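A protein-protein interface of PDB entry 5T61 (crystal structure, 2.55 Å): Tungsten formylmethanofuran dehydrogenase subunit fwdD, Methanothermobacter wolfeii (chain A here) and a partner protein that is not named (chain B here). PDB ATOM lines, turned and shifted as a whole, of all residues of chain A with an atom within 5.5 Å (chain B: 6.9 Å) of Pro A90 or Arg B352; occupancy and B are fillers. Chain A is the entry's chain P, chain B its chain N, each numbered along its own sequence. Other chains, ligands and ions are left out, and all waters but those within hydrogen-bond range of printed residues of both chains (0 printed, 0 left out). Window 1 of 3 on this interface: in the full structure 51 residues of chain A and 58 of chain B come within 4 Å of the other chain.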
ATOM      1  N   TYR A  57      -0.455 -21.620 -10.056  1.00  0.00           N
ATOM      2  CA  TYR A  57       0.316 -20.473 -10.508  1.00  0.00           C
ATOM      3  C   TYR A  57      -0.446 -19.157 -10.476  1.00  0.00           C
ATOM      4  O   TYR A  57       0.184 -18.100 -10.572  1.00  0.00           O
ATOM      5  CB  TYR A  57       0.832 -20.734 -11.927  1.00  0.00           C
ATOM      6  CG  TYR A  57       1.381 -22.135 -12.078  1.00  0.00           C
ATOM      7  CD1 TYR A  57       2.591 -22.488 -11.503  1.00  0.00           C
ATOM      8  CD2 TYR A  57       0.679 -23.108 -12.783  1.00  0.00           C
ATOM      9  CE1 TYR A  57       3.097 -23.767 -11.631  1.00  0.00           C
ATOM     10  CE2 TYR A  57       1.178 -24.392 -12.919  1.00  0.00           C
ATOM     11  CZ  TYR A  57       2.388 -24.716 -12.338  1.00  0.00           C
ATOM     12  OH  TYR A  57       2.899 -25.988 -12.466  1.00  0.00           O
ATOM     13  N   ILE A  88      -2.026 -20.380 -16.401  1.00  0.00           N
ATOM     14  CA  ILE A  88      -1.317 -21.504 -17.018  1.00  0.00           C
ATOM     15  C   ILE A  88       0.097 -21.608 -16.452  1.00  0.00           C
ATOM     16  O   ILE A  88       0.538 -20.740 -15.691  1.00  0.00           O
ATOM     17  CB  ILE A  88      -1.300 -21.410 -18.561  1.00  0.00           C
ATOM     18  CG1 ILE A  88      -0.727 -20.080 -19.057  1.00  0.00           C
ATOM     19  CG2 ILE A  88      -2.697 -21.655 -19.128  1.00  0.00           C
ATOM     20  CD1 ILE A  88       0.786 -20.072 -19.223  1.00  0.00           C
ATOM     21  N   ARG A  89       0.816 -22.665 -16.835  1.00  0.00           N
ATOM     22  CA  ARG A  89       2.102 -23.008 -16.222  1.00  0.00           C
ATOM     23  C   ARG A  89       3.241 -22.205 -16.843  1.00  0.00           C
ATOM     24  O   ARG A  89       3.429 -22.258 -18.065  1.00  0.00           O
ATOM     25  CB  ARG A  89       2.373 -24.502 -16.365  1.00  0.00           C
ATOM     26  CG  ARG A  89       3.813 -24.924 -16.096  1.00  0.00           C
ATOM     27  CD  ARG A  89       3.909 -26.437 -15.937  1.00  0.00           C
ATOM     28  NE  ARG A  89       5.226 -26.875 -15.483  1.00  0.00           N
ATOM     29  CZ  ARG A  89       6.211 -27.249 -16.296  1.00  0.00           C
ATOM     30  NH1 ARG A  89       6.025 -27.240 -17.609  1.00  0.00           N
ATOM     31  NH2 ARG A  89       7.380 -27.634 -15.800  1.00  0.00           N
ATOM     32  N   PRO A  90       4.019 -21.456 -16.048  1.00  0.00           N
ATOM     33  CA  PRO A  90       5.038 -20.565 -16.625  1.00  0.00           C
ATOM     34  C   PRO A  90       6.323 -21.263 -17.044  1.00  0.00           C
ATOM     35  O   PRO A  90       6.988 -20.831 -17.992  1.00  0.00           O
ATOM     36  CB  PRO A  90       5.316 -19.586 -15.480  1.00  0.00           C
ATOM     37  CG  PRO A  90       5.111 -20.423 -14.248  1.00  0.00           C
ATOM     38  CD  PRO A  90       4.004 -21.402 -14.574  1.00  0.00           C
ATOM     39  N   TYR A  91       6.683 -22.333 -16.339  1.00  0.00           N
ATOM     40  CA  TYR A  91       7.992 -22.946 -16.518  1.00  0.00           C
ATOM     41  C   TYR A  91       8.177 -23.482 -17.933  1.00  0.00           C
ATOM     42  O   TYR A  91       7.245 -24.006 -18.549  1.00  0.00           O
ATOM     43  CB  TYR A  91       8.192 -24.062 -15.494  1.00  0.00           C
ATOM     44  CG  TYR A  91       8.101 -23.573 -14.068  1.00  0.00           C
ATOM     45  CD1 TYR A  91       9.138 -22.843 -13.499  1.00  0.00           C
ATOM     46  CD2 TYR A  91       6.973 -23.820 -13.297  1.00  0.00           C
ATOM     47  CE1 TYR A  91       9.059 -22.387 -12.198  1.00  0.00           C
ATOM     48  CE2 TYR A  91       6.887 -23.365 -11.994  1.00  0.00           C
ATOM     49  CZ  TYR A  91       7.932 -22.650 -11.448  1.00  0.00           C
ATOM     50  OH  TYR A  91       7.851 -22.196 -10.151  1.00  0.00           O
ATOM     51  N   THR A  92       9.397 -23.336 -18.444  1.00  0.00           N
ATOM     52  CA  THR A  92       9.727 -23.695 -19.813  1.00  0.00           C
ATOM     53  C   THR A  92      10.516 -24.992 -19.924  1.00  0.00           C
ATOM     54  O   THR A  92      10.780 -25.440 -21.045  1.00  0.00           O
ATOM     55  CB  THR A  92      10.527 -22.564 -20.466  1.00  0.00           C
ATOM     56  OG1 THR A  92      11.876 -22.615 -19.985  1.00  0.00           O
ATOM     57  CG2 THR A  92       9.924 -21.218 -20.115  1.00  0.00           C
ATOM     58  N   THR A  97      10.044 -21.873 -23.850  1.00  0.00           N
ATOM     59  CA  THR A  97       8.621 -21.841 -24.173  1.00  0.00           C
ATOM     60  C   THR A  97       7.790 -22.301 -22.986  1.00  0.00           C
ATOM     61  O   THR A  97       7.934 -23.455 -22.551  1.00  0.00           O
ATOM     62  CB  THR A  97       8.336 -22.722 -25.384  1.00  0.00           C
ATOM     63  OG1 THR A  97       9.115 -22.269 -26.498  1.00  0.00           O
ATOM     64  CG2 THR A  97       6.863 -22.673 -25.750  1.00  0.00           C
ATOM     65  N   PRO A  98       6.904 -21.462 -22.450  1.00  0.00           N
ATOM     66  CA  PRO A  98       6.063 -21.878 -21.317  1.00  0.00           C
ATOM     67  C   PRO A  98       5.080 -22.977 -21.703  1.00  0.00           C
ATOM     68  O   PRO A  98       4.867 -23.292 -22.877  1.00  0.00           O
ATOM     69  CB  PRO A  98       5.321 -20.594 -20.928  1.00  0.00           C
ATOM     70  CG  PRO A  98       6.101 -19.479 -21.552  1.00  0.00           C
ATOM     71  CD  PRO A  98       6.702 -20.047 -22.799  1.00  0.00           C
ATOM     72  N   SER A  99       4.459 -23.556 -20.672  1.00  0.00           N
ATOM     73  CA  SER A  99       3.439 -24.594 -20.847  1.00  0.00           C
ATOM     74  C   SER A  99       2.062 -23.935 -20.854  1.00  0.00           C
ATOM     75  O   SER A  99       1.333 -23.922 -19.859  1.00  0.00           O
ATOM     76  CB  SER A  99       3.552 -25.649 -19.753  1.00  0.00           C
ATOM     77  OG  SER A  99       4.835 -26.242 -19.749  1.00  0.00           O
ATOM     78  N   LYS B 262       7.193 -30.683 -25.633  1.00  0.00           N
ATOM     79  CA  LYS B 262       7.516 -29.507 -26.435  1.00  0.00           C
ATOM     80  C   LYS B 262       8.379 -29.847 -27.645  1.00  0.00           C
ATOM     81  O   LYS B 262       7.883 -30.450 -28.604  1.00  0.00           O
ATOM     82  CB  LYS B 262       8.181 -28.453 -25.544  1.00  0.00           C
ATOM     83  CG  LYS B 262       7.194 -27.914 -24.511  1.00  0.00           C
ATOM     84  CD  LYS B 262       7.806 -27.014 -23.459  1.00  0.00           C
ATOM     85  CE  LYS B 262       6.710 -26.526 -22.517  1.00  0.00           C
ATOM     86  NZ  LYS B 262       7.233 -25.917 -21.262  1.00  0.00           N
ATOM     87  N   ASN B 327      11.396 -15.580 -21.959  1.00  0.00           N
ATOM     88  CA  ASN B 327      10.799 -16.033 -20.707  1.00  0.00           C
ATOM     89  C   ASN B 327      11.842 -16.520 -19.713  1.00  0.00           C
ATOM     90  O   ASN B 327      11.613 -16.450 -18.501  1.00  0.00           O
ATOM     91  CB  ASN B 327       9.763 -17.122 -20.973  1.00  0.00           C
ATOM     92  CG  ASN B 327       8.466 -16.561 -21.500  1.00  0.00           C
ATOM     93  OD1 ASN B 327       7.519 -16.351 -20.746  1.00  0.00           O
ATOM     94  ND2 ASN B 327       8.421 -16.294 -22.796  1.00  0.00           N
ATOM     95  N   LEU B 330      13.323 -13.232 -18.092  1.00  0.00           N
ATOM     96  CA  LEU B 330      12.321 -12.577 -17.255  1.00  0.00           C
ATOM     97  C   LEU B 330      11.998 -13.403 -16.010  1.00  0.00           C
ATOM     98  O   LEU B 330      12.028 -12.885 -14.889  1.00  0.00           O
ATOM     99  CB  LEU B 330      11.044 -12.287 -18.063  1.00  0.00           C
ATOM    100  CG  LEU B 330      11.108 -11.204 -19.146  1.00  0.00           C
ATOM    101  CD1 LEU B 330       9.841 -11.191 -19.992  1.00  0.00           C
ATOM    102  CD2 LEU B 330      11.328  -9.838 -18.504  1.00  0.00           C
ATOM    103  N   GLN B 331      11.695 -14.695 -16.180  1.00  0.00           N
ATOM    104  CA  GLN B 331      11.288 -15.498 -15.024  1.00  0.00           C
ATOM    105  C   GLN B 331      12.429 -15.744 -14.045  1.00  0.00           C
ATOM    106  O   GLN B 331      12.185 -15.883 -12.842  1.00  0.00           O
ATOM    107  CB  GLN B 331      10.703 -16.836 -15.475  1.00  0.00           C
ATOM    108  CG  GLN B 331       9.448 -16.723 -16.319  1.00  0.00           C
ATOM    109  CD  GLN B 331       8.842 -18.077 -16.627  1.00  0.00           C
ATOM    110  OE1 GLN B 331       9.037 -19.041 -15.882  1.00  0.00           O
ATOM    111  NE2 GLN B 331       8.097 -18.158 -17.721  1.00  0.00           N
ATOM    112  N   ASN B 332      13.668 -15.825 -14.523  1.00  0.00           N
ATOM    113  CA  ASN B 332      14.809 -15.929 -13.622  1.00  0.00           C
ATOM    114  C   ASN B 332      15.368 -14.571 -13.219  1.00  0.00           C
ATOM    115  O   ASN B 332      16.395 -14.521 -12.529  1.00  0.00           O
ATOM    116  CB  ASN B 332      15.906 -16.815 -14.240  1.00  0.00           C
ATOM    117  CG  ASN B 332      15.407 -18.225 -14.515  1.00  0.00           C
ATOM    118  OD1 ASN B 332      14.596 -18.767 -13.759  1.00  0.00           O
ATOM    119  ND2 ASN B 332      15.886 -18.826 -15.593  1.00  0.00           N
ATOM    120  N   ARG B 333      14.729 -13.473 -13.645  1.00  0.00           N
ATOM    121  CA  ARG B 333      15.060 -12.131 -13.175  1.00  0.00           C
ATOM    122  C   ARG B 333      16.452 -11.681 -13.611  1.00  0.00           C
ATOM    123  O   ARG B 333      17.072 -10.835 -12.962  1.00  0.00           O
ATOM    124  CB  ARG B 333      14.902 -12.066 -11.654  1.00  0.00           C
ATOM    125  CG  ARG B 333      13.505 -12.478 -11.199  1.00  0.00           C
ATOM    126  CD  ARG B 333      13.403 -12.610  -9.697  1.00  0.00           C
ATOM    127  NE  ARG B 333      13.942 -11.464  -8.973  1.00  0.00           N
ATOM    128  CZ  ARG B 333      13.329 -10.301  -8.804  1.00  0.00           C
ATOM    129  NH1 ARG B 333      12.123 -10.101  -9.307  1.00  0.00           N
ATOM    130  NH2 ARG B 333      13.927  -9.340  -8.114  1.00  0.00           N
ATOM    131  N   PHE B 349       2.513 -13.379 -22.305  1.00  0.00           N
ATOM    132  CA  PHE B 349       3.452 -14.101 -21.460  1.00  0.00           C
ATOM    133  C   PHE B 349       2.753 -14.601 -20.199  1.00  0.00           C
ATOM    134  O   PHE B 349       1.707 -14.076 -19.806  1.00  0.00           O
ATOM    135  CB  PHE B 349       4.646 -13.209 -21.085  1.00  0.00           C
ATOM    136  CG  PHE B 349       5.740 -13.177 -22.122  1.00  0.00           C
ATOM    137  CD1 PHE B 349       5.511 -13.625 -23.413  1.00  0.00           C
ATOM    138  CD2 PHE B 349       7.005 -12.705 -21.798  1.00  0.00           C
ATOM    139  CE1 PHE B 349       6.522 -13.600 -24.365  1.00  0.00           C
ATOM    140  CE2 PHE B 349       8.018 -12.678 -22.745  1.00  0.00           C
ATOM    141  CZ  PHE B 349       7.775 -13.125 -24.029  1.00  0.00           C
ATOM    142  N   PRO B 350       3.290 -15.632 -19.548  1.00  0.00           N
ATOM    143  CA  PRO B 350       2.689 -16.125 -18.302  1.00  0.00           C
ATOM    144  C   PRO B 350       2.915 -15.186 -17.123  1.00  0.00           C
ATOM    145  O   PRO B 350       3.771 -14.300 -17.147  1.00  0.00           O
ATOM    146  CB  PRO B 350       3.394 -17.466 -18.069  1.00  0.00           C
ATOM    147  CG  PRO B 350       4.668 -17.363 -18.799  1.00  0.00           C
ATOM    148  CD  PRO B 350       4.438 -16.453 -19.969  1.00  0.00           C
ATOM    149  N   GLN B 351       2.111 -15.415 -16.077  1.00  0.00           N
ATOM    150  CA  GLN B 351       2.128 -14.605 -14.862  1.00  0.00           C
ATOM    151  C   GLN B 351       3.539 -14.297 -14.365  1.00  0.00           C
ATOM    152  O   GLN B 351       3.865 -13.147 -14.052  1.00  0.00           O
ATOM    153  CB  GLN B 351       1.324 -15.317 -13.759  1.00  0.00           C
ATOM    154  CG  GLN B 351       1.930 -16.628 -13.230  1.00  0.00           C
ATOM    155  CD  GLN B 351       1.643 -17.818 -14.117  1.00  0.00           C
ATOM    156  OE1 GLN B 351       2.557 -18.501 -14.572  1.00  0.00           O
ATOM    157  NE2 GLN B 351       0.365 -18.092 -14.348  1.00  0.00           N
ATOM    158  N   ARG B 352       4.391 -15.321 -14.301  1.00  0.00           N
ATOM    159  CA  ARG B 352       5.694 -15.188 -13.672  1.00  0.00           C
ATOM    160  C   ARG B 352       6.589 -14.220 -14.433  1.00  0.00           C
ATOM    161  O   ARG B 352       7.406 -13.520 -13.823  1.00  0.00           O
ATOM    162  CB  ARG B 352       6.331 -16.571 -13.570  1.00  0.00           C
ATOM    163  CG  ARG B 352       7.539 -16.676 -12.679  1.00  0.00           C
ATOM    164  CD  ARG B 352       7.547 -18.053 -12.040  1.00  0.00           C
ATOM    165  NE  ARG B 352       8.694 -18.236 -11.163  1.00  0.00           N
ATOM    166  CZ  ARG B 352       9.862 -18.723 -11.564  1.00  0.00           C
ATOM    167  NH1 ARG B 352      10.036 -19.076 -12.831  1.00  0.00           N
ATOM    168  NH2 ARG B 352      10.859 -18.856 -10.698  1.00  0.00           N
ATOM    169  N   ALA B 353       6.440 -14.158 -15.758  1.00  0.00           N
ATOM    170  CA  ALA B 353       7.214 -13.212 -16.552  1.00  0.00           C
ATOM    171  C   ALA B 353       6.679 -11.794 -16.396  1.00  0.00           C
ATOM    172  O   ALA B 353       7.457 -10.834 -16.357  1.00  0.00           O
ATOM    173  CB  ALA B 353       7.212 -13.633 -18.020  1.00  0.00           C
ATOM    174  N   LEU B 354       5.355 -11.641 -16.317  1.00  0.00           N
ATOM    175  CA  LEU B 354       4.776 -10.317 -16.109  1.00  0.00           C
ATOM    176  C   LEU B 354       5.223  -9.718 -14.784  1.00  0.00           C
ATOM    177  O   LEU B 354       5.397  -8.498 -14.676  1.00  0.00           O
ATOM    178  CB  LEU B 354       3.249 -10.385 -16.167  1.00  0.00           C
ATOM    179  CG  LEU B 354       2.557 -10.077 -17.497  1.00  0.00           C
ATOM    180  CD1 LEU B 354       2.708  -8.600 -17.817  1.00  0.00           C
ATOM    181  CD2 LEU B 354       3.120 -10.920 -18.619  1.00  0.00           C
ATOM    182  N   GLU B 355       5.416 -10.559 -13.764  1.00  0.00           N
ATOM    183  CA  GLU B 355       5.862 -10.064 -12.462  1.00  0.00           C
ATOM    184  C   GLU B 355       7.196  -9.340 -12.569  1.00  0.00           C
ATOM    185  O   GLU B 355       7.453  -8.391 -11.817  1.00  0.00           O
ATOM    186  CB  GLU B 355       5.955 -11.226 -11.472  1.00  0.00           C
ATOM    187  CG  GLU B 355       4.623 -11.572 -10.828  1.00  0.00           C
ATOM    188  CD  GLU B 355       4.607 -12.953 -10.207  1.00  0.00           C
ATOM    189  OE1 GLU B 355       5.623 -13.342  -9.591  1.00  0.00           O
ATOM    190  OE2 GLU B 355       3.575 -13.648 -10.339  1.00  0.00           O
ATOM    191  N   ARG B 356       8.032  -9.754 -13.523  1.00  0.00           N
ATOM    192  CA  ARG B 356       9.341  -9.161 -13.711  1.00  0.00           C
ATOM    193  C   ARG B 356       9.256  -7.897 -14.562  1.00  0.00           C
ATOM    194  O   ARG B 356       9.972  -6.919 -14.307  1.00  0.00           O
ATOM    195  CB  ARG B 356      10.267 -10.210 -14.348  1.00  0.00           C
ATOM    196  CG  ARG B 356      11.667  -9.700 -14.699  1.00  0.00           C
ATOM    197  CD  ARG B 356      12.483  -9.411 -13.402  1.00  0.00           C
ATOM    198  NE  ARG B 356      13.811  -8.908 -13.713  1.00  0.00           N
ATOM    199  CZ  ARG B 356      14.589  -8.282 -12.837  1.00  0.00           C
ATOM    200  NH1 ARG B 356      14.205  -8.042 -11.568  1.00  0.00           N
ATOM    201  NH2 ARG B 356      15.786  -7.837 -13.211  1.00  0.00           N
ATOM    202  N   MET B 357       8.347  -7.890 -15.542  1.00  0.00           N
ATOM    203  CA  MET B 357       8.120  -6.691 -16.336  1.00  0.00           C
ATOM    204  C   MET B 357       7.655  -5.538 -15.467  1.00  0.00           C
ATOM    205  O   MET B 357       7.925  -4.375 -15.785  1.00  0.00           O
ATOM    206  CB  MET B 357       7.099  -6.966 -17.444  1.00  0.00           C
ATOM    207  CG  MET B 357       7.672  -7.627 -18.689  1.00  0.00           C
ATOM    208  SD  MET B 357       6.369  -8.177 -19.813  1.00  0.00           S
ATOM    209  CE  MET B 357       5.852  -6.626 -20.547  1.00  0.00           C
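OE1 of Gln B331 lies within hydrogen-bond range of NH1 of Arg B352 (3.2 Å). The guanidinium group (NH1) of Arg A89 sits at hydrogen-bond distance from the side-chain hydroxyl (OG) of Ser A99, 2.6 Å away. O of Tyr A91 sits at hydrogen-bond distance from OG of Ser A99 (3.5 Å).
Among the printed residues, pairs that only touch across the chains: Tyr A57 with Gln B351, Ile A88 with Pro B350, Pro A90 with Pro B350, Pro A90 with Gln B351, Pro A90 with Arg B352, Tyr A91 with Arg B352, Thr A92 with Lys B262, Pro A98 with Lys B262, Pro A98 with Asn B327 and Pro A98 with Pro B350.
Of chain B, only Gln B331, Pro B350, Gln B351 and Arg B352 come within 4 Å of Pro A90. Of chain A, only Pro A90 (3.7 Å) and Tyr A91 (3.5 Å) come within 4 Å of Arg B352. Printed residues of chain B within 4 Å of Tyr A91: Lys B262 (3.3 Å) and Arg B352 (3.5 Å). Printed residues of chain A within 4 Å of Asn B327: Pro A98. Of the printed residues of chain A, Gln B351 touches Tyr A57, Ile A88 and Pro A90. Of the printed residues of chain B, Pro A98 touches Lys B262 (3.7 Å), Asn B327 (3.5 Å) and Pro B350 (3.8 Å). Met B357 touches none of the printed residues of chain A. The nearest printed residue of chain A that does not touch Arg B352 is Tyr A57 (6.3 Å).
O of Tyr A91 lies within hydrogen-bond range of NZ of Lys B262, at 3.3 Å. NZ of Lys B262 sits at hydrogen-bond distance from O of Thr A97, at 2.9 Å. The side-chain amino group (NZ) of Lys B262 lies within hydrogen-bond range of the side-chain hydroxyl (OG) of Ser A99, at 2.9 Å. The side-chain amide nitrogen (NE2) of Gln B331 is in hydrogen-bond range of the backbone carbonyl oxygen (O) of Pro A90, 2.9 Å away. NE2 of Gln B351 lies within hydrogen-bond range of O of Ile A88, at 3.0 Å.
Printed residues of chain B that touch a printed residue of chain A: Lys B262, Asn B327, Gln B331, Pro B350, Gln B351 and Arg B352. Hydrophobic or aromatic side chains of chain B that line the printed part of chain A: Pro B350. Among the printed residues, 15 pairs touch across the chains. Among the printed residues, no Asp or Glu carboxylate lies within 4 Å of a Lys or Arg side-chain nitrogen of the other chain.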
